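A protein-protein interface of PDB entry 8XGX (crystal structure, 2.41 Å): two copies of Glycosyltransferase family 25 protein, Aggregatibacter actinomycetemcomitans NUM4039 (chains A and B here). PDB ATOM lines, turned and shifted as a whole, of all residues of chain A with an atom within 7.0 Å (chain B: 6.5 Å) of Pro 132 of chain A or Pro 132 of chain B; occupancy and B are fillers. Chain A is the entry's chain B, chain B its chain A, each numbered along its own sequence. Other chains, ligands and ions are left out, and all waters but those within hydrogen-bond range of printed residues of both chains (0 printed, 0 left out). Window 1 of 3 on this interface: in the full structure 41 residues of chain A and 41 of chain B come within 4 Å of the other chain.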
ATOM      1  N   PHE A 129     -21.992   2.434 -18.698  1.00  0.00           N
ATOM      2  CA  PHE A 129     -20.844   1.666 -19.260  1.00  0.00           C
ATOM      3  C   PHE A 129     -19.563   2.499 -19.105  1.00  0.00           C
ATOM      4  O   PHE A 129     -19.588   3.672 -19.492  1.00  0.00           O
ATOM      5  CB  PHE A 129     -21.089   1.272 -20.723  1.00  0.00           C
ATOM      6  CG  PHE A 129     -20.865   2.387 -21.711  1.00  0.00           C
ATOM      7  CD1 PHE A 129     -21.811   3.389 -21.874  1.00  0.00           C
ATOM      8  CD2 PHE A 129     -19.688   2.462 -22.442  1.00  0.00           C
ATOM      9  CE1 PHE A 129     -21.591   4.434 -22.762  1.00  0.00           C
ATOM     10  CE2 PHE A 129     -19.472   3.504 -23.332  1.00  0.00           C
ATOM     11  CZ  PHE A 129     -20.425   4.487 -23.494  1.00  0.00           C
ATOM     12  N   LEU A 130     -18.478   1.901 -18.615  1.00  0.00           N
ATOM     13  CA  LEU A 130     -17.134   2.536 -18.567  1.00  0.00           C
ATOM     14  C   LEU A 130     -16.146   1.809 -19.496  1.00  0.00           C
ATOM     15  O   LEU A 130     -16.370   0.633 -19.857  1.00  0.00           O
ATOM     16  CB  LEU A 130     -16.625   2.559 -17.119  1.00  0.00           C
ATOM     17  CG  LEU A 130     -17.127   3.722 -16.259  1.00  0.00           C
ATOM     18  CD1 LEU A 130     -16.615   3.589 -14.830  1.00  0.00           C
ATOM     19  CD2 LEU A 130     -16.715   5.069 -16.845  1.00  0.00           C
ATOM     20  N   MET A 131     -15.062   2.515 -19.822  1.00  0.00           N
ATOM     21  CA  MET A 131     -14.001   2.134 -20.787  1.00  0.00           C
ATOM     22  C   MET A 131     -13.381   0.801 -20.374  1.00  0.00           C
ATOM     23  O   MET A 131     -13.053   0.605 -19.210  1.00  0.00           O
ATOM     24  CB  MET A 131     -12.923   3.223 -20.797  1.00  0.00           C
ATOM     25  CG  MET A 131     -12.052   3.241 -22.031  1.00  0.00           C
ATOM     26  SD  MET A 131     -11.062   4.765 -22.083  1.00  0.00           S
ATOM     27  CE  MET A 131     -10.422   4.840 -20.409  1.00  0.00           C
ATOM     28  N   PRO A 132     -13.218  -0.169 -21.302  1.00  0.00           N
ATOM     29  CA  PRO A 132     -12.562  -1.436 -20.982  1.00  0.00           C
ATOM     30  C   PRO A 132     -11.112  -1.306 -20.488  1.00  0.00           C
ATOM     31  O   PRO A 132     -10.798  -1.844 -19.447  1.00  0.00           O
ATOM     32  CB  PRO A 132     -12.551  -2.220 -22.314  1.00  0.00           C
ATOM     33  CG  PRO A 132     -12.847  -1.202 -23.390  1.00  0.00           C
ATOM     34  CD  PRO A 132     -13.658  -0.121 -22.705  1.00  0.00           C
ATOM     35  N   VAL A 133     -10.266  -0.621 -21.259  1.00  0.00           N
ATOM     36  CA  VAL A 133      -8.792  -0.571 -21.054  1.00  0.00           C
ATOM     37  C   VAL A 133      -8.415   0.852 -20.633  1.00  0.00           C
ATOM     38  O   VAL A 133      -8.930   1.802 -21.244  1.00  0.00           O
ATOM     39  CB  VAL A 133      -8.047  -1.027 -22.323  1.00  0.00           C
ATOM     40  CG1 VAL A 133      -6.541  -1.008 -22.123  1.00  0.00           C
ATOM     41  CG2 VAL A 133      -8.518  -2.400 -22.780  1.00  0.00           C
ATOM     42  N   GLN A 134      -7.560   0.988 -19.618  1.00  0.00           N
ATOM     43  CA  GLN A 134      -7.034   2.297 -19.158  1.00  0.00           C
ATOM     44  C   GLN A 134      -5.501   2.288 -19.204  1.00  0.00           C
ATOM     45  O   GLN A 134      -4.893   1.190 -19.135  1.00  0.00           O
ATOM     46  CB  GLN A 134      -7.552   2.609 -17.755  1.00  0.00           C
ATOM     47  CG  GLN A 134      -9.066   2.538 -17.661  1.00  0.00           C
ATOM     48  CD  GLN A 134      -9.589   3.108 -16.366  1.00  0.00           C
ATOM     49  OE1 GLN A 134      -8.840   3.343 -15.417  1.00  0.00           O
ATOM     50  NE2 GLN A 134     -10.892   3.343 -16.333  1.00  0.00           N
ATOM     51  N   THR A 153      -4.231  -1.516 -18.670  1.00  0.00           N
ATOM     52  CA  THR A 153      -4.944  -2.396 -17.701  1.00  0.00           C
ATOM     53  C   THR A 153      -6.439  -2.394 -18.023  1.00  0.00           C
ATOM     54  O   THR A 153      -6.870  -1.552 -18.821  1.00  0.00           O
ATOM     55  CB  THR A 153      -4.711  -1.964 -16.247  1.00  0.00           C
ATOM     56  OG1 THR A 153      -4.700  -0.538 -16.213  1.00  0.00           O
ATOM     57  CG2 THR A 153      -3.424  -2.498 -15.667  1.00  0.00           C
ATOM     58  N   SER A 154      -7.175  -3.340 -17.446  1.00  0.00           N
ATOM     59  CA  SER A 154      -8.662  -3.380 -17.419  1.00  0.00           C
ATOM     60  C   SER A 154      -9.085  -4.124 -16.147  1.00  0.00           C
ATOM     61  O   SER A 154      -8.662  -5.291 -16.012  1.00  0.00           O
ATOM     62  CB  SER A 154      -9.235  -4.022 -18.678  1.00  0.00           C
ATOM     63  OG  SER A 154      -8.687  -5.310 -18.916  1.00  0.00           O
ATOM     64  N   LYS A 155      -9.864  -3.486 -15.259  1.00  0.00           N
ATOM     65  CA  LYS A 155     -10.161  -4.027 -13.900  1.00  0.00           C
ATOM     66  C   LYS A 155     -11.668  -4.103 -13.599  1.00  0.00           C
ATOM     67  O   LYS A 155     -12.067  -5.077 -12.913  1.00  0.00           O
ATOM     68  CB  LYS A 155      -9.409  -3.207 -12.846  1.00  0.00           C
ATOM     69  CG  LYS A 155      -7.892  -3.387 -12.864  1.00  0.00           C
ATOM     70  CD  LYS A 155      -7.223  -3.241 -11.499  1.00  0.00           C
ATOM     71  CE  LYS A 155      -5.778  -3.695 -11.483  1.00  0.00           C
ATOM     72  NZ  LYS A 155      -5.281  -3.896 -10.101  1.00  0.00           N
ATOM     73  N   HIS A 156     -12.477  -3.152 -14.078  1.00  0.00           N
ATOM     74  CA  HIS A 156     -13.886  -2.981 -13.627  1.00  0.00           C
ATOM     75  C   HIS A 156     -14.810  -2.434 -14.735  1.00  0.00           C
ATOM     76  O   HIS A 156     -14.735  -1.217 -15.016  1.00  0.00           O
ATOM     77  CB  HIS A 156     -13.887  -2.089 -12.379  1.00  0.00           C
ATOM     78  CG  HIS A 156     -15.265  -1.757 -11.919  1.00  0.00           C
ATOM     79  ND1 HIS A 156     -16.054  -2.683 -11.268  1.00  0.00           N
ATOM     80  CD2 HIS A 156     -16.018  -0.642 -12.057  1.00  0.00           C
ATOM     81  CE1 HIS A 156     -17.224  -2.148 -10.993  1.00  0.00           C
ATOM     82  NE2 HIS A 156     -17.231  -0.895 -11.473  1.00  0.00           N
ATOM     83  N   PHE A 157     -15.687  -3.293 -15.286  1.00  0.00           N
ATOM     84  CA  PHE A 157     -16.778  -2.960 -16.250  1.00  0.00           C
ATOM     85  C   PHE A 157     -18.106  -2.742 -15.517  1.00  0.00           C
ATOM     86  O   PHE A 157     -18.968  -2.010 -16.047  1.00  0.00           O
ATOM     87  CB  PHE A 157     -16.966  -4.084 -17.274  1.00  0.00           C
ATOM     88  CG  PHE A 157     -15.803  -4.231 -18.214  1.00  0.00           C
ATOM     89  CD1 PHE A 157     -14.697  -5.001 -17.876  1.00  0.00           C
ATOM     90  CD2 PHE A 157     -15.818  -3.574 -19.429  1.00  0.00           C
ATOM     91  CE1 PHE A 157     -13.621  -5.105 -18.741  1.00  0.00           C
ATOM     92  CE2 PHE A 157     -14.749  -3.689 -20.296  1.00  0.00           C
ATOM     93  CZ  PHE A 157     -13.649  -4.445 -19.948  1.00  0.00           C
ATOM     94  N   PHE A 192     -19.206  -8.746 -19.917  1.00  0.00           N
ATOM     95  CA  PHE A 192     -19.290  -7.421 -20.589  1.00  0.00           C
ATOM     96  C   PHE A 192     -18.024  -7.095 -21.394  1.00  0.00           C
ATOM     97  O   PHE A 192     -17.891  -5.934 -21.827  1.00  0.00           O
ATOM     98  CB  PHE A 192     -19.593  -6.338 -19.551  1.00  0.00           C
ATOM     99  CG  PHE A 192     -20.897  -6.561 -18.828  1.00  0.00           C
ATOM    100  CD1 PHE A 192     -22.076  -6.758 -19.527  1.00  0.00           C
ATOM    101  CD2 PHE A 192     -20.936  -6.606 -17.449  1.00  0.00           C
ATOM    102  CE1 PHE A 192     -23.269  -6.969 -18.856  1.00  0.00           C
ATOM    103  CE2 PHE A 192     -22.138  -6.794 -16.781  1.00  0.00           C
ATOM    104  CZ  PHE A 192     -23.298  -6.983 -17.483  1.00  0.00           C
ATOM    105  N   ASN A 193     -17.131  -8.059 -21.622  1.00  0.00           N
ATOM    106  CA  ASN A 193     -15.949  -7.818 -22.486  1.00  0.00           C
ATOM    107  C   ASN A 193     -15.724  -9.028 -23.386  1.00  0.00           C
ATOM    108  O   ASN A 193     -16.059  -8.948 -24.559  1.00  0.00           O
ATOM    109  CB  ASN A 193     -14.704  -7.441 -21.676  1.00  0.00           C
ATOM    110  CG  ASN A 193     -13.605  -6.856 -22.540  1.00  0.00           C
ATOM    111  OD1 ASN A 193     -13.835  -6.508 -23.699  1.00  0.00           O
ATOM    112  ND2 ASN A 193     -12.419  -6.709 -21.981  1.00  0.00           N
ATOM    113  N   PHE B 129      -3.340   5.926 -28.309  1.00  0.00           N
ATOM    114  CA  PHE B 129      -4.299   5.084 -27.561  1.00  0.00           C
ATOM    115  C   PHE B 129      -5.692   5.414 -28.086  1.00  0.00           C
ATOM    116  O   PHE B 129      -5.947   6.619 -28.289  1.00  0.00           O
ATOM    117  CB  PHE B 129      -4.193   5.343 -26.062  1.00  0.00           C
ATOM    118  CG  PHE B 129      -5.230   4.597 -25.268  1.00  0.00           C
ATOM    119  CD1 PHE B 129      -5.133   3.223 -25.101  1.00  0.00           C
ATOM    120  CD2 PHE B 129      -6.322   5.260 -24.732  1.00  0.00           C
ATOM    121  CE1 PHE B 129      -6.092   2.529 -24.383  1.00  0.00           C
ATOM    122  CE2 PHE B 129      -7.281   4.564 -24.012  1.00  0.00           C
ATOM    123  CZ  PHE B 129      -7.164   3.200 -23.841  1.00  0.00           C
ATOM    124  N   LEU B 130      -6.502   4.404 -28.421  1.00  0.00           N
ATOM    125  CA  LEU B 130      -7.831   4.607 -29.059  1.00  0.00           C
ATOM    126  C   LEU B 130      -8.924   4.118 -28.102  1.00  0.00           C
ATOM    127  O   LEU B 130      -8.798   2.988 -27.602  1.00  0.00           O
ATOM    128  CB  LEU B 130      -7.879   3.867 -30.402  1.00  0.00           C
ATOM    129  CG  LEU B 130      -7.236   4.593 -31.587  1.00  0.00           C
ATOM    130  CD1 LEU B 130      -7.221   3.709 -32.828  1.00  0.00           C
ATOM    131  CD2 LEU B 130      -7.945   5.912 -31.875  1.00  0.00           C
ATOM    132  N   MET B 131      -9.930   4.958 -27.833  1.00  0.00           N
ATOM    133  CA  MET B 131     -11.175   4.542 -27.124  1.00  0.00           C
ATOM    134  C   MET B 131     -11.918   3.583 -28.055  1.00  0.00           C
ATOM    135  O   MET B 131     -12.099   3.891 -29.231  1.00  0.00           O
ATOM    136  CB  MET B 131     -12.093   5.727 -26.792  1.00  0.00           C
ATOM    137  CG  MET B 131     -11.397   6.942 -26.175  1.00  0.00           C
ATOM    138  SD  MET B 131     -11.204   6.869 -24.372  1.00  0.00           S
ATOM    139  CE  MET B 131      -9.950   8.127 -24.121  1.00  0.00           C
ATOM    140  N   PRO B 132     -12.344   2.382 -27.600  1.00  0.00           N
ATOM    141  CA  PRO B 132     -13.127   1.504 -28.470  1.00  0.00           C
ATOM    142  C   PRO B 132     -14.511   2.122 -28.777  1.00  0.00           C
ATOM    143  O   PRO B 132     -15.007   2.932 -27.984  1.00  0.00           O
ATOM    144  CB  PRO B 132     -13.170   0.169 -27.695  1.00  0.00           C
ATOM    145  CG  PRO B 132     -12.908   0.541 -26.241  1.00  0.00           C
ATOM    146  CD  PRO B 132     -12.079   1.808 -26.267  1.00  0.00           C
ATOM    147  N   VAL B 133     -15.076   1.798 -29.947  1.00  0.00           N
ATOM    148  CA  VAL B 133     -16.527   2.008 -30.242  1.00  0.00           C
ATOM    149  C   VAL B 133     -17.303   1.010 -29.373  1.00  0.00           C
ATOM    150  O   VAL B 133     -16.919  -0.183 -29.348  1.00  0.00           O
ATOM    151  CB  VAL B 133     -16.848   1.868 -31.745  1.00  0.00           C
ATOM    152  CG1 VAL B 133     -18.347   1.779 -32.022  1.00  0.00           C
ATOM    153  CG2 VAL B 133     -16.230   3.009 -32.547  1.00  0.00           C
ATOM    154  N   GLN B 134     -18.316   1.492 -28.648  1.00  0.00           N
ATOM    155  CA  GLN B 134     -19.015   0.700 -27.605  1.00  0.00           C
ATOM    156  C   GLN B 134     -20.530   0.671 -27.853  1.00  0.00           C
ATOM    157  O   GLN B 134     -21.097  -0.408 -27.714  1.00  0.00           O
ATOM    158  CB  GLN B 134     -18.639   1.218 -26.216  1.00  0.00           C
ATOM    159  CG  GLN B 134     -17.137   1.193 -25.970  1.00  0.00           C
ATOM    160  CD  GLN B 134     -16.760   1.416 -24.526  1.00  0.00           C
ATOM    161  OE1 GLN B 134     -16.145   2.423 -24.170  1.00  0.00           O
ATOM    162  NE2 GLN B 134     -17.120   0.465 -23.677  1.00  0.00           N
ATOM    163  N   LEU B 135     -21.193   1.792 -28.121  1.00  0.00           N
ATOM    164  CA  LEU B 135     -22.675   1.789 -28.266  1.00  0.00           C
ATOM    165  C   LEU B 135     -23.051   1.837 -29.746  1.00  0.00           C
ATOM    166  O   LEU B 135     -22.805   2.875 -30.371  1.00  0.00           O
ATOM    167  CB  LEU B 135     -23.256   2.973 -27.492  1.00  0.00           C
ATOM    168  CG  LEU B 135     -22.968   2.967 -25.993  1.00  0.00           C
ATOM    169  CD1 LEU B 135     -23.769   4.053 -25.291  1.00  0.00           C
ATOM    170  CD2 LEU B 135     -23.257   1.607 -25.376  1.00  0.00           C
ATOM    171  N   THR B 153     -20.744  -3.176 -28.032  1.00  0.00           N
ATOM    172  CA  THR B 153     -19.569  -3.787 -28.716  1.00  0.00           C
ATOM    173  C   THR B 153     -18.294  -3.262 -28.042  1.00  0.00           C
ATOM    174  O   THR B 153     -18.408  -2.383 -27.165  1.00  0.00           O
ATOM    175  CB  THR B 153     -19.578  -3.487 -30.219  1.00  0.00           C
ATOM    176  OG1 THR B 153     -20.018  -2.138 -30.399  1.00  0.00           O
ATOM    177  CG2 THR B 153     -20.469  -4.424 -31.007  1.00  0.00           C
ATOM    178  N   SER B 154     -17.124  -3.774 -28.413  1.00  0.00           N
ATOM    179  CA  SER B 154     -15.825  -3.082 -28.194  1.00  0.00           C
ATOM    180  C   SER B 154     -14.945  -3.343 -29.419  1.00  0.00           C
ATOM    181  O   SER B 154     -14.435  -4.464 -29.562  1.00  0.00           O
ATOM    182  CB  SER B 154     -15.178  -3.460 -26.886  1.00  0.00           C
ATOM    183  OG  SER B 154     -15.079  -4.866 -26.760  1.00  0.00           O
ATOM    184  N   LYS B 155     -14.860  -2.346 -30.305  1.00  0.00           N
ATOM    185  CA  LYS B 155     -14.352  -2.489 -31.695  1.00  0.00           C
ATOM    186  C   LYS B 155     -13.337  -1.381 -31.986  1.00  0.00           C
ATOM    187  O   LYS B 155     -13.426  -0.324 -31.349  1.00  0.00           O
ATOM    188  CB  LYS B 155     -15.525  -2.449 -32.679  1.00  0.00           C
ATOM    189  CG  LYS B 155     -16.450  -3.659 -32.623  1.00  0.00           C
ATOM    190  CD  LYS B 155     -17.488  -3.682 -33.724  1.00  0.00           C
ATOM    191  CE  LYS B 155     -18.334  -2.423 -33.791  1.00  0.00           C
ATOM    192  NZ  LYS B 155     -19.289  -2.452 -34.926  1.00  0.00           N
ATOM    193  N   HIS B 156     -12.411  -1.644 -32.914  1.00  0.00           N
ATOM    194  CA  HIS B 156     -11.418  -0.689 -33.484  1.00  0.00           C
ATOM    195  C   HIS B 156     -10.556  -0.094 -32.358  1.00  0.00           C
ATOM    196  O   HIS B 156     -10.803   1.060 -31.942  1.00  0.00           O
ATOM    197  CB  HIS B 156     -12.098   0.342 -34.402  1.00  0.00           C
ATOM    198  CG  HIS B 156     -13.113  -0.250 -35.324  1.00  0.00           C
ATOM    199  ND1 HIS B 156     -12.790  -1.185 -36.295  1.00  0.00           N
ATOM    200  CD2 HIS B 156     -14.444  -0.041 -35.430  1.00  0.00           C
ATOM    201  CE1 HIS B 156     -13.880  -1.528 -36.953  1.00  0.00           C
ATOM    202  NE2 HIS B 156     -14.910  -0.833 -36.445  1.00  0.00           N
ATOM    203  N   PHE B 157      -9.573  -0.880 -31.898  1.00  0.00           N
ATOM    204  CA  PHE B 157      -8.520  -0.497 -30.915  1.00  0.00           C
ATOM    205  C   PHE B 157      -7.240  -0.054 -31.637  1.00  0.00           C
ATOM    206  O   PHE B 157      -6.483   0.731 -31.047  1.00  0.00           O
ATOM    207  CB  PHE B 157      -8.205  -1.659 -29.977  1.00  0.00           C
ATOM    208  CG  PHE B 157      -9.337  -2.052 -29.064  1.00  0.00           C
ATOM    209  CD1 PHE B 157     -10.287  -2.973 -29.472  1.00  0.00           C
ATOM    210  CD2 PHE B 157      -9.462  -1.483 -27.804  1.00  0.00           C
ATOM    211  CE1 PHE B 157     -11.329  -3.328 -28.628  1.00  0.00           C
ATOM    212  CE2 PHE B 157     -10.505  -1.843 -26.962  1.00  0.00           C
ATOM    213  CZ  PHE B 157     -11.432  -2.771 -27.373  1.00  0.00           C
ATOM    214  N   ASN B 193      -7.279  -5.815 -26.097  1.00  0.00           N
ATOM    215  CA  ASN B 193      -8.432  -5.857 -25.160  1.00  0.00           C
ATOM    216  C   ASN B 193      -8.384  -7.172 -24.381  1.00  0.00           C
ATOM    217  O   ASN B 193      -7.984  -7.147 -23.235  1.00  0.00           O
ATOM    218  CB  ASN B 193      -9.758  -5.626 -25.892  1.00  0.00           C
ATOM    219  CG  ASN B 193     -10.934  -5.399 -24.965  1.00  0.00           C
ATOM    220  OD1 ASN B 193     -10.761  -5.215 -23.758  1.00  0.00           O
ATOM    221  ND2 ASN B 193     -12.134  -5.409 -25.518  1.00  0.00           N
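Leu 130 of chain A touches Gln 134 of chain B, but with the chains exchanged Gln 134 of chain A does not touch Leu 130 of chain B (8.3 Å). Pro 132 of chain A touches Gln 134 of chain B, but with the chains exchanged Gln 134 of chain A does not touch Pro 132 of chain B (8.1 Å). Val 133 of chain A touches Phe 129 of chain B, but with the chains exchanged Phe 129 of chain A does not touch Val 133 of chain B (6.9 Å). Asn 193 of chain A touches its own counterpart, Asn 193 of chain B. Of the 11 pairs that touch across the chains among the printed residues, 3 have their exchanged pair printed and touching as well.
Hydrophobic or aromatic side chains of chain A that line the printed part of chain B: Phe 129, Met 131, Pro 132 and Val 133. Printed residues of chain B that touch a printed residue of chain A: Phe 129, Met 131, Pro 132, Gln 134, Leu 135, Ser 154 and Asn 193. Among the printed residues, no Asp or Glu carboxylate lies within 4 Å of a Lys or Arg side-chain nitrogen of the other chain.
Gln 134 of chain B touches Phe 129 of chain A (NE2 to CD2, 3.5 Å). Leu 135 of chain B touches Phe 129 of chain A. O of Leu 130 of chain A touches NE2 of Gln 134 of chain B (3.9 Å). Pro 132 of chain B touches Pro 132 of chain A. NE2 of Gln 134 of chain B touches CD of Pro 132 of chain A, at 3.6 Å. Pro 132 of chain A touches Asn 193 of chain B. Val 133 of chain A touches Phe 129 of chain B. Asn 193 of chain B touches Val 133 of chain A. Ser 154 of chain B touches Asn 193 of chain A (OG to OD1, 3.7 Å).
OD1 of Asn 193 of chain A sits at hydrogen-bond distance from ND2 of Asn 193 of chain B. The side-chain sulfur (SD) of Met 131 of chain A sits close to the side-chain sulfur (SD) of Met 131 of chain B.
The backbone carbonyl oxygen (O) of Gln 134 of chain B lies within hydrogen-bond range of the backbone NH (N) of Thr 153 of chain B. The side-chain amide nitrogen (ND2) of Asn 193 of chain B lies within hydrogen-bond range of the side-chain hydroxyl (OG) of Ser 154 of chain B (3.2 Å).
Pro 132 of chain A touches just these residues of chain B: Pro 132 (3.3 Å), Gln 134 (3.6 Å) and Asn 193 (3.8 Å). Of chain A, only Pro 132 comes within 4 Å of Pro 132 of chain B. Printed residues of chain B within 4 Å of Met 131 of chain A: Met 131. Of the printed residues of chain B, Phe 129 of chain A touches Gln 134 and Leu 135. Printed residues of chain A within 4 Å of Ser 154 of chain B: Asn 193. Of the printed residues of chain B, Leu 130 of chain A touches Gln 134. Lys 155 of chain B touches none of the printed residues of chain A. Lys 155 of chain A touches none of the printed residues of chain B. The nearest residue of chain B that does not touch Pro 132 of chain A is Phe 157 of chain B (4.3 Å). The nearest printed residue of chain A that does not touch Met 131 of chain B is Val 133 of chain A (6.4 Å).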
